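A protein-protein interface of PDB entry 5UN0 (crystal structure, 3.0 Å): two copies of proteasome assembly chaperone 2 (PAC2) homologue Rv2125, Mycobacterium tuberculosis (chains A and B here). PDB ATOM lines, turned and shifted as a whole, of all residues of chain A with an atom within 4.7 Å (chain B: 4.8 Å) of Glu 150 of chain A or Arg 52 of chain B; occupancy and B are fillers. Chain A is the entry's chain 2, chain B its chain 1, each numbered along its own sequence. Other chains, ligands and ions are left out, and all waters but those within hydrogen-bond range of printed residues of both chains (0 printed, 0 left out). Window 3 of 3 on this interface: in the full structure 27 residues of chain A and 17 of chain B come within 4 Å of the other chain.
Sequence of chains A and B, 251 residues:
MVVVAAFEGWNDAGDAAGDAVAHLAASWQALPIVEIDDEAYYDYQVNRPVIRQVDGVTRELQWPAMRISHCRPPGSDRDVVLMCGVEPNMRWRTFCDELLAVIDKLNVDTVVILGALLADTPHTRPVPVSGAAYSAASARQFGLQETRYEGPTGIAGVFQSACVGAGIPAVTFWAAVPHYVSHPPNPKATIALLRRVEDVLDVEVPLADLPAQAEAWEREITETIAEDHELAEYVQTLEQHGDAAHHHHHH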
ATOM      1  N   ARG A 148       0.267 -26.380   4.713  1.00  0.00           N
ATOM      2  CA  ARG A 148       0.056 -25.150   3.896  1.00  0.00           C
ATOM      3  C   ARG A 148      -0.875 -25.411   2.705  1.00  0.00           C
ATOM      4  O   ARG A 148      -0.448 -25.889   1.655  1.00  0.00           O
ATOM      5  CB  ARG A 148       1.355 -24.461   3.420  1.00  0.00           C
ATOM      6  CG  ARG A 148       1.735 -24.749   1.970  1.00  0.00           C
ATOM      7  CD  ARG A 148       3.144 -25.268   1.790  1.00  0.00           C
ATOM      8  NE  ARG A 148       3.377 -25.779   0.418  1.00  0.00           N
ATOM      9  CZ  ARG A 148       3.156 -27.035  -0.010  1.00  0.00           C
ATOM     10  NH1 ARG A 148       2.688 -27.960   0.798  1.00  0.00           N
ATOM     11  NH2 ARG A 148       3.394 -27.370  -1.275  1.00  0.00           N
ATOM     12  N   TYR A 149      -2.149 -25.086   2.878  1.00  0.00           N
ATOM     13  CA  TYR A 149      -3.081 -25.044   1.756  1.00  0.00           C
ATOM     14  C   TYR A 149      -2.699 -23.842   0.909  1.00  0.00           C
ATOM     15  O   TYR A 149      -2.763 -23.894  -0.323  1.00  0.00           O
ATOM     16  CB  TYR A 149      -4.510 -24.846   2.219  1.00  0.00           C
ATOM     17  CG  TYR A 149      -5.065 -25.957   3.031  1.00  0.00           C
ATOM     18  CD1 TYR A 149      -6.003 -26.832   2.493  1.00  0.00           C
ATOM     19  CD2 TYR A 149      -4.680 -26.114   4.358  1.00  0.00           C
ATOM     20  CE1 TYR A 149      -6.526 -27.852   3.255  1.00  0.00           C
ATOM     21  CE2 TYR A 149      -5.204 -27.119   5.135  1.00  0.00           C
ATOM     22  CZ  TYR A 149      -6.125 -27.987   4.585  1.00  0.00           C
ATOM     23  OH  TYR A 149      -6.637 -28.983   5.379  1.00  0.00           O
ATOM     24  N   GLU A 150      -2.361 -22.748   1.602  1.00  0.00           N
ATOM     25  CA  GLU A 150      -1.727 -21.579   1.007  1.00  0.00           C
ATOM     26  C   GLU A 150      -0.461 -21.254   1.805  1.00  0.00           C
ATOM     27  O   GLU A 150      -0.475 -21.253   3.036  1.00  0.00           O
ATOM     28  CB  GLU A 150      -2.677 -20.372   0.962  1.00  0.00           C
ATOM     29  CG  GLU A 150      -2.086 -19.134   0.273  1.00  0.00           C
ATOM     30  CD  GLU A 150      -3.119 -18.295  -0.460  1.00  0.00           C
ATOM     31  OE1 GLU A 150      -4.274 -18.246   0.003  1.00  0.00           O
ATOM     32  OE2 GLU A 150      -2.773 -17.683  -1.498  1.00  0.00           O
ATOM     33  N   GLY A 151       0.633 -21.011   1.086  1.00  0.00           N
ATOM     34  CA  GLY A 151       1.936 -20.737   1.685  1.00  0.00           C
ATOM     35  C   GLY A 151       3.083 -21.299   0.851  1.00  0.00           C
ATOM     36  O   GLY A 151       2.847 -21.869  -0.207  1.00  0.00           O
ATOM     37  N   VAL B  50       4.916 -19.965  -3.718  1.00  0.00           N
ATOM     38  CA  VAL B  50       3.721 -20.060  -2.897  1.00  0.00           C
ATOM     39  C   VAL B  50       2.713 -20.946  -3.601  1.00  0.00           C
ATOM     40  O   VAL B  50       2.359 -20.702  -4.761  1.00  0.00           O
ATOM     41  CB  VAL B  50       3.105 -18.676  -2.614  1.00  0.00           C
ATOM     42  CG1 VAL B  50       2.024 -18.785  -1.553  1.00  0.00           C
ATOM     43  CG2 VAL B  50       4.170 -17.695  -2.145  1.00  0.00           C
ATOM     44  N   ILE B  51       2.284 -21.985  -2.887  1.00  0.00           N
ATOM     45  CA  ILE B  51       1.268 -22.911  -3.375  1.00  0.00           C
ATOM     46  C   ILE B  51      -0.077 -22.524  -2.786  1.00  0.00           C
ATOM     47  O   ILE B  51      -0.142 -22.021  -1.665  1.00  0.00           O
ATOM     48  CB  ILE B  51       1.580 -24.375  -2.987  1.00  0.00           C
ATOM     49  CG1 ILE B  51       0.999 -25.339  -4.034  1.00  0.00           C
ATOM     50  CG2 ILE B  51       1.074 -24.721  -1.588  1.00  0.00           C
ATOM     51  CD1 ILE B  51       2.054 -26.170  -4.709  1.00  0.00           C
ATOM     52  N   ARG B  52      -1.144 -22.752  -3.550  1.00  0.00           N
ATOM     53  CA  ARG B  52      -2.504 -22.633  -3.032  1.00  0.00           C
ATOM     54  C   ARG B  52      -3.259 -23.904  -3.378  1.00  0.00           C
ATOM     55  O   ARG B  52      -3.471 -24.195  -4.548  1.00  0.00           O
ATOM     56  CB  ARG B  52      -3.227 -21.415  -3.600  1.00  0.00           C
ATOM     57  CG  ARG B  52      -4.492 -21.041  -2.825  1.00  0.00           C
ATOM     58  CD  ARG B  52      -4.994 -19.652  -3.195  1.00  0.00           C
ATOM     59  NE  ARG B  52      -5.308 -19.556  -4.622  1.00  0.00           N
ATOM     60  CZ  ARG B  52      -6.417 -20.031  -5.190  1.00  0.00           C
ATOM     61  NH1 ARG B  52      -7.349 -20.645  -4.458  1.00  0.00           N
ATOM     62  NH2 ARG B  52      -6.594 -19.891  -6.497  1.00  0.00           N
ATOM     63  N   GLN B  53      -3.661 -24.648  -2.345  1.00  0.00           N
ATOM     64  CA  GLN B  53      -4.360 -25.929  -2.504  1.00  0.00           C
ATOM     65  C   GLN B  53      -5.694 -25.938  -1.794  1.00  0.00           C
ATOM     66  O   GLN B  53      -5.795 -25.587  -0.611  1.00  0.00           O
ATOM     67  CB  GLN B  53      -3.539 -27.079  -1.943  1.00  0.00           C
ATOM     68  CG  GLN B  53      -2.107 -27.087  -2.411  1.00  0.00           C
ATOM     69  CD  GLN B  53      -1.335 -28.240  -1.844  1.00  0.00           C
ATOM     70  OE1 GLN B  53      -0.868 -29.091  -2.577  1.00  0.00           O
ATOM     71  NE2 GLN B  53      -1.208 -28.279  -0.523  1.00  0.00           N
ATOM     72  N   VAL B  54      -6.709 -26.373  -2.530  1.00  0.00           N
ATOM     73  CA  VAL B  54      -8.080 -26.384  -2.049  1.00  0.00           C
ATOM     74  C   VAL B  54      -8.694 -27.758  -2.326  1.00  0.00           C
ATOM     75  O   VAL B  54      -8.713 -28.223  -3.470  1.00  0.00           O
ATOM     76  CB  VAL B  54      -8.923 -25.274  -2.728  1.00  0.00           C
ATOM     77  CG1 VAL B  54     -10.357 -25.290  -2.219  1.00  0.00           C
ATOM     78  CG2 VAL B  54      -8.295 -23.904  -2.509  1.00  0.00           C
ATOM     79  N   VAL B  57      -6.572 -30.424  -4.130  1.00  0.00           N
ATOM     80  CA  VAL B  57      -5.913 -30.041  -5.382  1.00  0.00           C
ATOM     81  C   VAL B  57      -5.241 -28.683  -5.300  1.00  0.00           C
ATOM     82  O   VAL B  57      -5.777 -27.749  -4.701  1.00  0.00           O
ATOM     83  CB  VAL B  57      -6.876 -30.078  -6.597  1.00  0.00           C
ATOM     84  CG1 VAL B  57      -7.352 -31.495  -6.830  1.00  0.00           C
ATOM     85  CG2 VAL B  57      -8.065 -29.146  -6.413  1.00  0.00           C
ATOM     86  N   THR B  58      -4.073 -28.572  -5.925  1.00  0.00           N
ATOM     87  CA  THR B  58      -3.403 -27.283  -5.986  1.00  0.00           C
ATOM     88  C   THR B  58      -4.147 -26.468  -7.031  1.00  0.00           C
ATOM     89  O   THR B  58      -4.476 -26.975  -8.098  1.00  0.00           O
ATOM     90  CB  THR B  58      -1.884 -27.354  -6.300  1.00  0.00           C
ATOM     91  OG1 THR B  58      -1.662 -27.448  -7.712  1.00  0.00           O
ATOM     92  CG2 THR B  58      -1.224 -28.526  -5.596  1.00  0.00           C
ATOM     93  N   ARG B  59      -4.466 -25.231  -6.687  1.00  0.00           N
ATOM     94  CA  ARG B  59      -5.185 -24.346  -7.585  1.00  0.00           C
ATOM     95  C   ARG B  59      -4.304 -23.192  -8.066  1.00  0.00           C
ATOM     96  O   ARG B  59      -4.614 -22.542  -9.076  1.00  0.00           O
ATOM     97  CB  ARG B  59      -6.451 -23.793  -6.912  1.00  0.00           C
ATOM     98  CG  ARG B  59      -7.503 -24.840  -6.507  1.00  0.00           C
ATOM     99  CD  ARG B  59      -8.931 -24.424  -6.881  1.00  0.00           C
ATOM    100  NE  ARG B  59      -9.146 -22.969  -6.779  1.00  0.00           N
ATOM    101  CZ  ARG B  59     -10.187 -22.302  -7.274  1.00  0.00           C
ATOM    102  NH1 ARG B  59     -11.157 -22.940  -7.921  1.00  0.00           N
ATOM    103  NH2 ARG B  59     -10.248 -20.979  -7.120  1.00  0.00           N
ATOM    104  N   GLU B  60      -3.208 -22.926  -7.364  1.00  0.00           N
ATOM    105  CA  GLU B  60      -2.313 -21.865  -7.802  1.00  0.00           C
ATOM    106  C   GLU B  60      -0.872 -22.070  -7.352  1.00  0.00           C
ATOM    107  O   GLU B  60      -0.589 -22.547  -6.243  1.00  0.00           O
ATOM    108  CB  GLU B  60      -2.827 -20.505  -7.331  1.00  0.00           C
ATOM    109  CG  GLU B  60      -2.567 -19.384  -8.325  1.00  0.00           C
ATOM    110  CD  GLU B  60      -2.611 -18.005  -7.688  1.00  0.00           C
ATOM    111  OE1 GLU B  60      -1.755 -17.176  -8.030  1.00  0.00           O
ATOM    112  OE2 GLU B  60      -3.490 -17.757  -6.838  1.00  0.00           O
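Printed residues of chain B that touch a printed residue of chain A: Val 50, Ile 51, Arg 52 and Gln 53. Hydrophobic or aromatic side chains of chain B that line the printed part of chain A: Val 50 and Ile 51. Of the 4 printed residues of chain A, 4 touch a printed residue of chain B. Printed residues of chain A that touch a printed residue of chain B: Arg 148, Tyr 149, Glu 150 and Gly 151. Hydrophobic or aromatic side chains of chain A that line the printed part of chain B: Tyr 149. Among the printed residues, 9 pairs touch across the chains. Among the printed residues, no Asp or Glu carboxylate lies within 4 Å of a Lys or Arg side-chain nitrogen of the other chain.
Among the printed residues, pairs that only touch across the chains: Arg 148 of chain A with Ile 51 of chain B, Tyr 149 of chain A with Arg 52 of chain B, Glu 150 of chain A with Ile 51 of chain B, Glu 150 of chain A with Arg 52 of chain B and Gly 151 of chain A with Val 50 of chain B.
Of the printed residues of chain B, Arg 148 of chain A touches Ile 51 (3.2 Å) and Gln 53 (3.3 Å). Of chain B, only Ile 51 and Arg 52 come within 4 Å of Glu 150 of chain A. Printed residues of chain B within 4 Å of Gly 151 of chain A: Val 50 (3.4 Å) and Ile 51 (2.7 Å). Of the printed residues of chain A, Val 50 of chain B touches Gly 151 (3.4 Å). Arg 52 of chain B touches just these residues of chain A: Tyr 149 (3.0 Å) and Glu 150 (3.4 Å). Glu 60 of chain B touches none of the printed residues of chain A. The nearest residue of chain B that does not touch Glu 150 of chain A is Val 50 of chain B (4.5 Å).
NE of Arg 52 of chain B lies within salt-bridge range of OE2 of Glu 60 of chain B, at 3.4 Å. O of Arg 52 of chain B sits at hydrogen-bond distance from N of Arg 59 of chain B (2.6 Å).
No position is printed for both chains. Of the 9 pairs that touch across the chains among the printed residues, none has its exchanged pair printed and touching as well.
The backbone NH (N) of Gln 53 of chain B sits close to the backbone carbonyl oxygen (O) of Tyr 149 of chain A (2.3 Å). O of Gly 151 of chain A sits at hydrogen-bond distance from N of Ile 51 of chain B (2.7 Å). O of Ile 51 of chain B sits close to O of Tyr 149 of chain A (3.5 Å). NE2 of Gln 53 of chain B is in hydrogen-bond range of O of Arg 148 of chain A, at 3.3 Å.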
